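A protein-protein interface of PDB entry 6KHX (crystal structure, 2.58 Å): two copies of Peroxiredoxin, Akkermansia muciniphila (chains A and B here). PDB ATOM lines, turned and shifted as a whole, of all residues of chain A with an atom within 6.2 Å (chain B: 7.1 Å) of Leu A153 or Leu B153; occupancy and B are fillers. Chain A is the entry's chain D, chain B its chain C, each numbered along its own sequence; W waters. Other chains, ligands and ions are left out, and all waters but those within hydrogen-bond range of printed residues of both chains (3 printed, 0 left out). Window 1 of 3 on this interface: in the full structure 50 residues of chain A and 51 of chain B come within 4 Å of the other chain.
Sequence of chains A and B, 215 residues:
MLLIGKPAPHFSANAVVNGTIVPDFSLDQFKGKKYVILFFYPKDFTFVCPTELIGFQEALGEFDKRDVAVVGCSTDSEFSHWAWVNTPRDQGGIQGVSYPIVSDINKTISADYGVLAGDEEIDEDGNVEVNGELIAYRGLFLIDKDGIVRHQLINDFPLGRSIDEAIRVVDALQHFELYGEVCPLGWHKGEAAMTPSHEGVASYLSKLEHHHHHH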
ATOM      1  N   VAL A 115       5.881  -4.452 -29.838  1.00  0.00           N
ATOM      2  CA  VAL A 115       4.586  -4.971 -30.260  1.00  0.00           C
ATOM      3  C   VAL A 115       4.676  -5.867 -31.486  1.00  0.00           C
ATOM      4  O   VAL A 115       3.641  -6.343 -31.963  1.00  0.00           O
ATOM      5  CB  VAL A 115       3.579  -3.829 -30.511  1.00  0.00           C
ATOM      6  CG1 VAL A 115       3.402  -2.991 -29.250  1.00  0.00           C
ATOM      7  CG2 VAL A 115       4.013  -2.969 -31.699  1.00  0.00           C
ATOM      8  N   ARG A 138      -2.140  -5.420 -31.460  1.00  0.00           N
ATOM      9  CA  ARG A 138      -2.986  -4.258 -31.183  1.00  0.00           C
ATOM     10  C   ARG A 138      -2.426  -3.558 -29.950  1.00  0.00           C
ATOM     11  O   ARG A 138      -2.878  -3.742 -28.817  1.00  0.00           O
ATOM     12  CB  ARG A 138      -4.441  -4.674 -31.015  1.00  0.00           C
ATOM     13  CG  ARG A 138      -4.984  -5.316 -32.283  1.00  0.00           C
ATOM     14  CD  ARG A 138      -6.484  -5.546 -32.288  1.00  0.00           C
ATOM     15  NE  ARG A 138      -6.817  -6.479 -33.363  1.00  0.00           N
ATOM     16  CZ  ARG A 138      -6.884  -6.157 -34.651  1.00  0.00           C
ATOM     17  NH1 ARG A 138      -6.673  -4.908 -35.046  1.00  0.00           N
ATOM     18  NH2 ARG A 138      -7.173  -7.090 -35.546  1.00  0.00           N
ATOM     19  N   GLY A 139      -1.419  -2.729 -30.190  1.00  0.00           N
ATOM     20  CA  GLY A 139      -0.669  -2.079 -29.117  1.00  0.00           C
ATOM     21  C   GLY A 139      -1.048  -0.613 -29.013  1.00  0.00           C
ATOM     22  O   GLY A 139      -1.270   0.043 -30.026  1.00  0.00           O
ATOM     23  N   LEU A 140      -1.120  -0.096 -27.793  1.00  0.00           N
ATOM     24  CA  LEU A 140      -1.482   1.304 -27.624  1.00  0.00           C
ATOM     25  C   LEU A 140      -0.640   1.919 -26.520  1.00  0.00           C
ATOM     26  O   LEU A 140      -0.456   1.322 -25.456  1.00  0.00           O
ATOM     27  CB  LEU A 140      -2.974   1.472 -27.320  1.00  0.00           C
ATOM     28  CG  LEU A 140      -3.442   2.923 -27.169  1.00  0.00           C
ATOM     29  CD1 LEU A 140      -4.794   3.112 -27.827  1.00  0.00           C
ATOM     30  CD2 LEU A 140      -3.506   3.319 -25.697  1.00  0.00           C
ATOM     31  N   PHE A 141      -0.150   3.130 -26.778  1.00  0.00           N
ATOM     32  CA  PHE A 141       0.734   3.834 -25.867  1.00  0.00           C
ATOM     33  C   PHE A 141       0.242   5.255 -25.667  1.00  0.00           C
ATOM     34  O   PHE A 141      -0.157   5.928 -26.624  1.00  0.00           O
ATOM     35  CB  PHE A 141       2.181   3.863 -26.384  1.00  0.00           C
ATOM     36  CG  PHE A 141       2.756   2.505 -26.646  1.00  0.00           C
ATOM     37  CD1 PHE A 141       2.463   1.823 -27.815  1.00  0.00           C
ATOM     38  CD2 PHE A 141       3.578   1.902 -25.709  1.00  0.00           C
ATOM     39  CE1 PHE A 141       2.981   0.575 -28.046  1.00  0.00           C
ATOM     40  CE2 PHE A 141       4.100   0.650 -25.938  1.00  0.00           C
ATOM     41  CZ  PHE A 141       3.802  -0.014 -27.107  1.00  0.00           C
ATOM     42  N   HIS A 151       1.493   4.850 -20.194  1.00  0.00           N
ATOM     43  CA  HIS A 151       0.514   3.777 -20.212  1.00  0.00           C
ATOM     44  C   HIS A 151       0.720   2.979 -21.484  1.00  0.00           C
ATOM     45  O   HIS A 151       1.006   3.554 -22.541  1.00  0.00           O
ATOM     46  CB  HIS A 151      -0.914   4.330 -20.152  1.00  0.00           C
ATOM     47  CG  HIS A 151      -1.957   3.390 -20.670  1.00  0.00           C
ATOM     48  ND1 HIS A 151      -2.537   2.414 -19.885  1.00  0.00           N
ATOM     49  CD2 HIS A 151      -2.527   3.277 -21.892  1.00  0.00           C
ATOM     50  CE1 HIS A 151      -3.418   1.740 -20.602  1.00  0.00           C
ATOM     51  NE2 HIS A 151      -3.431   2.244 -21.824  1.00  0.00           N
ATOM     52  N   GLN A 152       0.621   1.657 -21.375  1.00  0.00           N
ATOM     53  CA  GLN A 152       0.672   0.822 -22.563  1.00  0.00           C
ATOM     54  C   GLN A 152      -0.261  -0.366 -22.394  1.00  0.00           C
ATOM     55  O   GLN A 152      -0.513  -0.837 -21.280  1.00  0.00           O
ATOM     56  CB  GLN A 152       2.085   0.320 -22.882  1.00  0.00           C
ATOM     57  CG  GLN A 152       2.671  -0.607 -21.855  1.00  0.00           C
ATOM     58  CD  GLN A 152       3.964  -1.218 -22.339  1.00  0.00           C
ATOM     59  OE1 GLN A 152       5.060  -0.747 -22.012  1.00  0.00           O
ATOM     60  NE2 GLN A 152       3.844  -2.248 -23.175  1.00  0.00           N
ATOM     61  N   LEU A 153      -0.747  -0.858 -23.527  1.00  0.00           N
ATOM     62  CA  LEU A 153      -1.741  -1.913 -23.580  1.00  0.00           C
ATOM     63  C   LEU A 153      -1.543  -2.650 -24.895  1.00  0.00           C
ATOM     64  O   LEU A 153      -1.356  -2.018 -25.939  1.00  0.00           O
ATOM     65  CB  LEU A 153      -3.155  -1.324 -23.471  1.00  0.00           C
ATOM     66  CG  LEU A 153      -4.430  -2.104 -23.805  1.00  0.00           C
ATOM     67  CD1 LEU A 153      -5.582  -1.449 -23.068  1.00  0.00           C
ATOM     68  CD2 LEU A 153      -4.729  -2.149 -25.298  1.00  0.00           C
ATOM     69  N   ILE A 154      -1.568  -3.978 -24.847  1.00  0.00           N
ATOM     70  CA  ILE A 154      -1.455  -4.792 -26.051  1.00  0.00           C
ATOM     71  C   ILE A 154      -2.529  -5.866 -26.003  1.00  0.00           C
ATOM     72  O   ILE A 154      -2.638  -6.598 -25.010  1.00  0.00           O
ATOM     73  CB  ILE A 154      -0.071  -5.450 -26.194  1.00  0.00           C
ATOM     74  CG1 ILE A 154       1.051  -4.451 -25.921  1.00  0.00           C
ATOM     75  CG2 ILE A 154       0.086  -6.000 -27.601  1.00  0.00           C
ATOM     76  CD1 ILE A 154       2.422  -5.082 -25.940  1.00  0.00           C
ATOM     77  N   ASN A 155      -3.300  -5.974 -27.082  1.00  0.00           N
ATOM     78  CA  ASN A 155      -4.337  -6.983 -27.221  1.00  0.00           C
ATOM     79  C   ASN A 155      -3.969  -7.954 -28.331  1.00  0.00           C
ATOM     80  O   ASN A 155      -3.321  -7.590 -29.318  1.00  0.00           O
ATOM     81  CB  ASN A 155      -5.704  -6.358 -27.525  1.00  0.00           C
ATOM     82  CG  ASN A 155      -6.368  -5.778 -26.293  1.00  0.00           C
ATOM     83  OD1 ASN A 155      -5.788  -5.773 -25.210  1.00  0.00           O
ATOM     84  ND2 ASN A 155      -7.595  -5.285 -26.454  1.00  0.00           N
ATOM     85  N   ARG A 161      -9.871  -2.843 -29.173  1.00  0.00           N
ATOM     86  CA  ARG A 161      -9.611  -1.999 -28.015  1.00  0.00           C
ATOM     87  C   ARG A 161     -10.820  -1.103 -27.725  1.00  0.00           C
ATOM     88  O   ARG A 161     -11.886  -1.233 -28.334  1.00  0.00           O
ATOM     89  CB  ARG A 161      -8.329  -1.205 -28.247  1.00  0.00           C
ATOM     90  CG  ARG A 161      -7.067  -2.050 -28.141  1.00  0.00           C
ATOM     91  CD  ARG A 161      -5.898  -1.402 -28.873  1.00  0.00           C
ATOM     92  NE  ARG A 161      -5.993  -1.573 -30.320  1.00  0.00           N
ATOM     93  CZ  ARG A 161      -5.021  -1.263 -31.173  1.00  0.00           C
ATOM     94  NH1 ARG A 161      -3.879  -0.766 -30.720  1.00  0.00           N
ATOM     95  NH2 ARG A 161      -5.188  -1.442 -32.479  1.00  0.00           N
ATOM     96  N   GLU A 165     -11.456   3.527 -22.529  1.00  0.00           N
ATOM     97  CA  GLU A 165     -10.328   3.303 -21.629  1.00  0.00           C
ATOM     98  C   GLU A 165      -9.162   4.228 -21.964  1.00  0.00           C
ATOM     99  O   GLU A 165      -8.470   4.715 -21.061  1.00  0.00           O
ATOM    100  CB  GLU A 165      -9.902   1.833 -21.675  1.00  0.00           C
ATOM    101  CG  GLU A 165      -8.787   1.465 -20.697  1.00  0.00           C
ATOM    102  CD  GLU A 165      -9.122   1.778 -19.238  1.00  0.00           C
ATOM    103  OE1 GLU A 165     -10.319   1.764 -18.861  1.00  0.00           O
ATOM    104  OE2 GLU A 165      -8.169   2.033 -18.464  1.00  0.00           O
ATOM    105  N   ILE B   4       2.118 -11.539 -25.470  1.00  0.00           N
ATOM    106  CA  ILE B   4       0.892 -11.841 -26.196  1.00  0.00           C
ATOM    107  C   ILE B   4       1.114 -13.047 -27.088  1.00  0.00           C
ATOM    108  O   ILE B   4       2.070 -13.096 -27.871  1.00  0.00           O
ATOM    109  CB  ILE B   4       0.437 -10.622 -27.008  1.00  0.00           C
ATOM    110  CG1 ILE B   4       0.118  -9.458 -26.070  1.00  0.00           C
ATOM    111  CG2 ILE B   4      -0.767 -10.981 -27.860  1.00  0.00           C
ATOM    112  CD1 ILE B   4      -1.035  -9.738 -25.124  1.00  0.00           C
ATOM    113  N   LEU B  38      -4.161 -11.611 -13.684  1.00  0.00           N
ATOM    114  CA  LEU B  38      -3.004 -11.450 -12.806  1.00  0.00           C
ATOM    115  C   LEU B  38      -2.562  -9.993 -12.832  1.00  0.00           C
ATOM    116  O   LEU B  38      -2.222  -9.467 -13.896  1.00  0.00           O
ATOM    117  CB  LEU B  38      -1.855 -12.359 -13.244  1.00  0.00           C
ATOM    118  CG  LEU B  38      -0.517 -12.142 -12.536  1.00  0.00           C
ATOM    119  CD1 LEU B  38      -0.580 -12.574 -11.066  1.00  0.00           C
ATOM    120  CD2 LEU B  38       0.601 -12.850 -13.288  1.00  0.00           C
ATOM    121  N   VAL B 115       7.392  -6.308 -15.943  1.00  0.00           N
ATOM    122  CA  VAL B 115       6.778  -5.216 -15.199  1.00  0.00           C
ATOM    123  C   VAL B 115       7.694  -4.639 -14.130  1.00  0.00           C
ATOM    124  O   VAL B 115       7.287  -3.719 -13.418  1.00  0.00           O
ATOM    125  CB  VAL B 115       5.437  -5.651 -14.566  1.00  0.00           C
ATOM    126  CG1 VAL B 115       4.471  -6.136 -15.637  1.00  0.00           C
ATOM    127  CG2 VAL B 115       5.652  -6.719 -13.498  1.00  0.00           C
ATOM    128  N   TYR B 137       5.551  -2.210 -11.716  1.00  0.00           N
ATOM    129  CA  TYR B 137       4.567  -1.259 -12.212  1.00  0.00           C
ATOM    130  C   TYR B 137       3.171  -1.876 -12.172  1.00  0.00           C
ATOM    131  O   TYR B 137       2.994  -3.070 -11.913  1.00  0.00           O
ATOM    132  CB  TYR B 137       4.901  -0.830 -13.638  1.00  0.00           C
ATOM    133  CG  TYR B 137       5.878   0.313 -13.743  1.00  0.00           C
ATOM    134  CD1 TYR B 137       5.530   1.590 -13.316  1.00  0.00           C
ATOM    135  CD2 TYR B 137       7.150   0.121 -14.265  1.00  0.00           C
ATOM    136  CE1 TYR B 137       6.422   2.644 -13.412  1.00  0.00           C
ATOM    137  CE2 TYR B 137       8.049   1.173 -14.365  1.00  0.00           C
ATOM    138  CZ  TYR B 137       7.678   2.430 -13.934  1.00  0.00           C
ATOM    139  OH  TYR B 137       8.561   3.478 -14.030  1.00  0.00           O
ATOM    140  N   ARG B 138       2.165  -1.050 -12.457  1.00  0.00           N
ATOM    141  CA  ARG B 138       0.776  -1.507 -12.416  1.00  0.00           C
ATOM    142  C   ARG B 138       0.500  -2.350 -13.656  1.00  0.00           C
ATOM    143  O   ARG B 138      -0.017  -1.886 -14.674  1.00  0.00           O
ATOM    144  CB  ARG B 138      -0.178  -0.330 -12.288  1.00  0.00           C
ATOM    145  CG  ARG B 138       0.036   0.399 -10.980  1.00  0.00           C
ATOM    146  CD  ARG B 138      -1.032   1.424 -10.644  1.00  0.00           C
ATOM    147  NE  ARG B 138      -0.536   2.245  -9.548  1.00  0.00           N
ATOM    148  CZ  ARG B 138      -0.506   1.843  -8.285  1.00  0.00           C
ATOM    149  NH1 ARG B 138      -0.970   0.643  -7.957  1.00  0.00           N
ATOM    150  NH2 ARG B 138      -0.012   2.637  -7.348  1.00  0.00           N
ATOM    151  N   GLY B 139       0.848  -3.626 -13.554  1.00  0.00           N
ATOM    152  CA  GLY B 139       0.791  -4.538 -14.693  1.00  0.00           C
ATOM    153  C   GLY B 139      -0.398  -5.474 -14.579  1.00  0.00           C
ATOM    154  O   GLY B 139      -0.745  -5.904 -13.483  1.00  0.00           O
ATOM    155  N   LEU B 140      -1.029  -5.781 -15.705  1.00  0.00           N
ATOM    156  CA  LEU B 140      -2.186  -6.666 -15.678  1.00  0.00           C
ATOM    157  C   LEU B 140      -2.162  -7.581 -16.891  1.00  0.00           C
ATOM    158  O   LEU B 140      -1.930  -7.128 -18.016  1.00  0.00           O
ATOM    159  CB  LEU B 140      -3.502  -5.869 -15.627  1.00  0.00           C
ATOM    160  CG  LEU B 140      -4.804  -6.664 -15.540  1.00  0.00           C
ATOM    161  CD1 LEU B 140      -5.781  -5.980 -14.590  1.00  0.00           C
ATOM    162  CD2 LEU B 140      -5.433  -6.851 -16.916  1.00  0.00           C
ATOM    163  N   PHE B 141      -2.432  -8.865 -16.658  1.00  0.00           N
ATOM    164  CA  PHE B 141      -2.383  -9.879 -17.700  1.00  0.00           C
ATOM    165  C   PHE B 141      -3.634 -10.738 -17.654  1.00  0.00           C
ATOM    166  O   PHE B 141      -4.057 -11.180 -16.578  1.00  0.00           O
ATOM    167  CB  PHE B 141      -1.133 -10.763 -17.565  1.00  0.00           C
ATOM    168  CG  PHE B 141       0.155  -9.990 -17.588  1.00  0.00           C
ATOM    169  CD1 PHE B 141       0.641  -9.379 -16.439  1.00  0.00           C
ATOM    170  CD2 PHE B 141       0.844  -9.815 -18.783  1.00  0.00           C
ATOM    171  CE1 PHE B 141       1.822  -8.652 -16.473  1.00  0.00           C
ATOM    172  CE2 PHE B 141       2.011  -9.085 -18.828  1.00  0.00           C
ATOM    173  CZ  PHE B 141       2.507  -8.504 -17.670  1.00  0.00           C
ATOM    174  N   LEU B 142      -4.212 -10.968 -18.832  1.00  0.00           N
ATOM    175  CA  LEU B 142      -5.292 -11.923 -19.026  1.00  0.00           C
ATOM    176  C   LEU B 142      -4.692 -13.191 -19.615  1.00  0.00           C
ATOM    177  O   LEU B 142      -4.058 -13.149 -20.677  1.00  0.00           O
ATOM    178  CB  LEU B 142      -6.373 -11.359 -19.948  1.00  0.00           C
ATOM    179  CG  LEU B 142      -7.499 -12.344 -20.280  1.00  0.00           C
ATOM    180  CD1 LEU B 142      -8.134 -12.877 -19.011  1.00  0.00           C
ATOM    181  CD2 LEU B 142      -8.542 -11.691 -21.172  1.00  0.00           C
ATOM    182  N   HIS B 151      -3.988 -10.570 -23.383  1.00  0.00           N
ATOM    183  CA  HIS B 151      -4.126  -9.139 -23.191  1.00  0.00           C
ATOM    184  C   HIS B 151      -3.169  -8.734 -22.087  1.00  0.00           C
ATOM    185  O   HIS B 151      -3.021  -9.458 -21.098  1.00  0.00           O
ATOM    186  CB  HIS B 151      -5.572  -8.786 -22.833  1.00  0.00           C
ATOM    187  CG  HIS B 151      -5.732  -7.489 -22.100  1.00  0.00           C
ATOM    188  ND1 HIS B 151      -5.846  -6.277 -22.743  1.00  0.00           N
ATOM    189  CD2 HIS B 151      -5.815  -7.220 -20.774  1.00  0.00           C
ATOM    190  CE1 HIS B 151      -5.988  -5.315 -21.848  1.00  0.00           C
ATOM    191  NE2 HIS B 151      -5.974  -5.861 -20.646  1.00  0.00           N
ATOM    192  N   GLN B 152      -2.497  -7.604 -22.270  1.00  0.00           N
ATOM    193  CA  GLN B 152      -1.631  -7.084 -21.226  1.00  0.00           C
ATOM    194  C   GLN B 152      -1.713  -5.566 -21.221  1.00  0.00           C
ATOM    195  O   GLN B 152      -1.952  -4.928 -22.252  1.00  0.00           O
ATOM    196  CB  GLN B 152      -0.174  -7.546 -21.393  1.00  0.00           C
ATOM    197  CG  GLN B 152       0.515  -7.064 -22.657  1.00  0.00           C
ATOM    198  CD  GLN B 152       1.996  -7.411 -22.673  1.00  0.00           C
ATOM    199  OE1 GLN B 152       2.410  -8.416 -23.262  1.00  0.00           O
ATOM    200  NE2 GLN B 152       2.801  -6.594 -21.994  1.00  0.00           N
ATOM    201  N   LEU B 153      -1.495  -5.001 -20.040  1.00  0.00           N
ATOM    202  CA  LEU B 153      -1.666  -3.584 -19.787  1.00  0.00           C
ATOM    203  C   LEU B 153      -0.745  -3.211 -18.639  1.00  0.00           C
ATOM    204  O   LEU B 153      -0.645  -3.954 -17.657  1.00  0.00           O
ATOM    205  CB  LEU B 153      -3.137  -3.281 -19.464  1.00  0.00           C
ATOM    206  CG  LEU B 153      -3.613  -1.983 -18.817  1.00  0.00           C
ATOM    207  CD1 LEU B 153      -5.060  -1.778 -19.184  1.00  0.00           C
ATOM    208  CD2 LEU B 153      -3.479  -2.029 -17.303  1.00  0.00           C
ATOM    209  N   ILE B 154      -0.044  -2.086 -18.776  1.00  0.00           N
ATOM    210  CA  ILE B 154       0.819  -1.575 -17.717  1.00  0.00           C
ATOM    211  C   ILE B 154       0.570  -0.078 -17.561  1.00  0.00           C
ATOM    212  O   ILE B 154       0.574   0.665 -18.551  1.00  0.00           O
ATOM    213  CB  ILE B 154       2.314  -1.839 -17.987  1.00  0.00           C
ATOM    214  CG1 ILE B 154       2.552  -3.284 -18.425  1.00  0.00           C
ATOM    215  CG2 ILE B 154       3.132  -1.542 -16.730  1.00  0.00           C
ATOM    216  CD1 ILE B 154       3.988  -3.577 -18.796  1.00  0.00           C
ATOM    217  N   ASN B 155       0.342   0.356 -16.322  1.00  0.00           N
ATOM    218  CA  ASN B 155       0.140   1.760 -15.995  1.00  0.00           C
ATOM    219  C   ASN B 155       1.269   2.277 -15.113  1.00  0.00           C
ATOM    220  O   ASN B 155       1.815   1.547 -14.280  1.00  0.00           O
ATOM    221  CB  ASN B 155      -1.191   1.984 -15.272  1.00  0.00           C
ATOM    222  CG  ASN B 155      -2.382   1.996 -16.213  1.00  0.00           C
ATOM    223  OD1 ASN B 155      -2.252   1.767 -17.420  1.00  0.00           O
ATOM    224  ND2 ASN B 155      -3.559   2.268 -15.657  1.00  0.00           N
ATOM    225  N   LEU B 159      -1.540   5.969 -11.813  1.00  0.00           N
ATOM    226  CA  LEU B 159      -2.704   5.771 -12.680  1.00  0.00           C
ATOM    227  C   LEU B 159      -3.350   4.421 -12.373  1.00  0.00           C
ATOM    228  O   LEU B 159      -2.934   3.389 -12.905  1.00  0.00           O
ATOM    229  CB  LEU B 159      -2.284   5.859 -14.144  1.00  0.00           C
ATOM    230  CG  LEU B 159      -1.402   7.068 -14.477  1.00  0.00           C
ATOM    231  CD1 LEU B 159      -1.077   7.129 -15.966  1.00  0.00           C
ATOM    232  CD2 LEU B 159      -2.060   8.367 -14.011  1.00  0.00           C
ATOM    233  N   GLY B 160      -4.398   4.437 -11.552  1.00  0.00           N
ATOM    234  CA  GLY B 160      -5.109   3.212 -11.244  1.00  0.00           C
ATOM    235  C   GLY B 160      -5.766   2.602 -12.468  1.00  0.00           C
ATOM    236  O   GLY B 160      -6.054   3.272 -13.460  1.00  0.00           O
ATOM    237  N   ARG B 161      -6.000   1.292 -12.391  1.00  0.00           N
ATOM    238  CA  ARG B 161      -6.548   0.542 -13.511  1.00  0.00           C
ATOM    239  C   ARG B 161      -8.075   0.536 -13.427  1.00  0.00           C
ATOM    240  O   ARG B 161      -8.674   1.185 -12.563  1.00  0.00           O
ATOM    241  CB  ARG B 161      -5.955  -0.864 -13.533  1.00  0.00           C
ATOM    242  CG  ARG B 161      -4.502  -0.895 -13.995  1.00  0.00           C
ATOM    243  CD  ARG B 161      -3.766  -2.138 -13.533  1.00  0.00           C
ATOM    244  NE  ARG B 161      -3.415  -2.059 -12.121  1.00  0.00           N
ATOM    245  CZ  ARG B 161      -2.576  -2.888 -11.512  1.00  0.00           C
ATOM    246  NH1 ARG B 161      -1.986  -3.852 -12.199  1.00  0.00           N
ATOM    247  NH2 ARG B 161      -2.314  -2.747 -10.219  1.00  0.00           N
ATOM    248  N   SER B 162      -8.722  -0.210 -14.319  1.00  0.00           N
ATOM    249  CA  SER B 162     -10.177  -0.222 -14.425  1.00  0.00           C
ATOM    250  C   SER B 162     -10.677  -1.656 -14.475  1.00  0.00           C
ATOM    251  O   SER B 162     -10.287  -2.421 -15.363  1.00  0.00           O
ATOM    252  CB  SER B 162     -10.645   0.529 -15.670  1.00  0.00           C
ATOM    253  OG  SER B 162     -11.898   0.027 -16.104  1.00  0.00           O
ATOM    254  N   GLU B 165     -12.690  -2.453 -17.813  1.00  0.00           N
ATOM    255  CA  GLU B 165     -11.912  -2.828 -18.990  1.00  0.00           C
ATOM    256  C   GLU B 165     -11.431  -4.273 -18.899  1.00  0.00           C
ATOM    257  O   GLU B 165     -11.405  -4.987 -19.909  1.00  0.00           O
ATOM    258  CB  GLU B 165     -10.731  -1.870 -19.175  1.00  0.00           C
ATOM    259  CG  GLU B 165      -9.920  -2.112 -20.453  1.00  0.00           C
ATOM    260  CD  GLU B 165     -10.750  -2.007 -21.736  1.00  0.00           C
ATOM    261  OE1 GLU B 165     -11.731  -1.228 -21.768  1.00  0.00           O
ATOM    262  OE2 GLU B 165     -10.428  -2.726 -22.709  1.00  0.00           O
ATOM    263  N   ALA B 166     -11.058  -4.726 -17.699  1.00  0.00           N
ATOM    264  CA  ALA B 166     -10.654  -6.119 -17.527  1.00  0.00           C
ATOM    265  C   ALA B 166     -11.807  -7.067 -17.838  1.00  0.00           C
ATOM    266  O   ALA B 166     -11.638  -8.058 -18.565  1.00  0.00           O
ATOM    267  CB  ALA B 166     -10.136  -6.344 -16.106  1.00  0.00           C
ATOM    268  N   ARG B 168     -14.351  -6.391 -19.709  1.00  0.00           N
ATOM    269  CA  ARG B 168     -14.662  -6.280 -21.130  1.00  0.00           C
ATOM    270  C   ARG B 168     -13.722  -7.136 -21.966  1.00  0.00           C
ATOM    271  O   ARG B 168     -14.154  -7.806 -22.910  1.00  0.00           O
ATOM    272  CB  ARG B 168     -14.588  -4.822 -21.577  1.00  0.00           C
ATOM    273  CG  ARG B 168     -15.147  -4.584 -22.970  1.00  0.00           C
ATOM    274  CD  ARG B 168     -14.786  -3.198 -23.472  1.00  0.00           C
ATOM    275  NE  ARG B 168     -13.392  -3.131 -23.891  1.00  0.00           N
ATOM    276  CZ  ARG B 168     -12.971  -3.448 -25.110  1.00  0.00           C
ATOM    277  NH1 ARG B 168     -13.840  -3.845 -26.030  1.00  0.00           N
ATOM    278  NH2 ARG B 168     -11.681  -3.368 -25.408  1.00  0.00           N
ATOM    279  N   VAL B 169     -12.427  -7.117 -21.637  1.00  0.00           N
ATOM    280  CA  VAL B 169     -11.468  -7.925 -22.381  1.00  0.00           C
ATOM    281  C   VAL B 169     -11.733  -9.409 -22.161  1.00  0.00           C
ATOM    282  O   VAL B 169     -11.628 -10.216 -23.095  1.00  0.00           O
ATOM    283  CB  VAL B 169     -10.029  -7.541 -21.996  1.00  0.00           C
ATOM    284  CG1 VAL B 169      -9.051  -8.418 -22.728  1.00  0.00           C
ATOM    285  CG2 VAL B 169      -9.767  -6.093 -22.337  1.00  0.00           C
HETATM  286  O   HOH W   1      -7.663  -0.395 -16.883  1.00  0.00           O
HETATM  287  O   HOH W   2       1.670  -3.945 -21.921  1.00  0.00           O
HETATM  288  O   HOH W   3      -5.584   1.669 -17.230  1.00  0.00           O
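Hydrophobic or aromatic side chains of chain B that line the printed part of chain A: Ile B4, His B151 and Leu B153.
Of the 12 printed residues of chain A, 7 touch a printed residue of chain B.
Printed residues of chain A that touch a printed residue of chain B: His A151, Gln A152, Leu A153, Ile A154, Asn A155, Arg A161 and Glu A165.
Among the printed residues, no Asp or Glu carboxylate lies within 4 Å of a Lys or Arg side-chain nitrogen of the other chain.
ND1 of His A151 lies within hydrogen-bond range of OD1 of Asn B155 (2.6 Å).
The backbone NH of Ile B154 lies within hydrogen-bond range of the backbone carbonyl oxygen of Gln A152, at 2.8 Å.
The backbone NH (N) of Ile A154 lies within hydrogen-bond range of the backbone carbonyl oxygen (O) of Gln B152, at 2.8 Å.
A ring nitrogen (ND1) of His B151 lies within hydrogen-bond range of the side-chain amide oxygen (OD1) of Asn A155 (2.5 Å).
Water W3 lies within hydrogen-bond range of the side-chain amide nitrogen (ND2) of Asn B155 (2.6 Å) and the side-chain carboxylate (OE2) of Glu A165 (2.9 Å).
Water W1 bridges N of Ser B162 (2.8 Å) and OE2 of Glu A165 (2.9 Å).
Water W2 lies within hydrogen-bond range of the side-chain amide nitrogen (NE2) of Gln B152 (2.9 Å) and the side-chain amide nitrogen (NE2) of Gln A152 (3.0 Å).
Val A115 touches none of the printed residues of chain B.
Printed residues of chain B within 4 Å of Asn A155: His B151 (2.5 Å).
Leu B153 touches just these residues of chain A: Gln A152 (3.3 Å) and Leu A153 (3.9 Å).
Of the printed residues of chain A, Asn B155 touches His A151.
Printed residues of chain A within 4 Å of Arg B168: Arg A161 (3.4 Å).
The nearest residue of chain B that does not touch Leu A153 is His B151 (4.1 Å).
The nearest residue of chain A that does not touch Leu B153 is His A151 (4.1 Å).
The nearest printed residue of chain B that does not touch Glu A165 is Leu B153 (5.0 Å).
His A151 touches Ile B154, and with the chains exchanged Ile A154 touches His B151.
His A151 touches Asn B155, and with the chains exchanged Asn A155 touches His B151.
Gln A152 touches Leu B153, and with the chains exchanged Leu A153 touches Gln B152.
Gln A152 touches Ile B154, and with the chains exchanged Ile A154 touches Gln B152.
Of the 13 pairs that touch across the chains among the printed residues, 10 have their exchanged pair printed and touching as well.
Among the printed residues, pairs that only touch across the chains: Leu A153 with Gln B152, Gln A152 with Leu B153, Arg A161 with Arg B168, Glu A165 with Ser B162, Ile A154 with His B151, Ile A154 with Ile B4, His A151 with Ile B154, Glu A165 with Glu B165 and Leu A153 with Leu B153.
ND2 of Asn B155 is in hydrogen-bond range of O of Gly B160, 3.5 Å away.
The backbone NH of Leu A140 sits at hydrogen-bond distance from the backbone carbonyl oxygen of Leu A153 (2.7 Å).
The backbone carbonyl oxygen (O) of Gly A139 is in hydrogen-bond range of the guanidinium group (NH1) of Arg A161 (2.8 Å).
The backbone carbonyl oxygen (O) of His B151 sits at hydrogen-bond distance from the backbone NH (N) of Leu B142 (3.0 Å).
O of Arg A138 is in hydrogen-bond range of N of Asn A155 (2.9 Å).
The side-chain carboxylate of Glu B165 is in salt-bridge range of the guanidinium group of Arg B168, 3.0 Å away.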
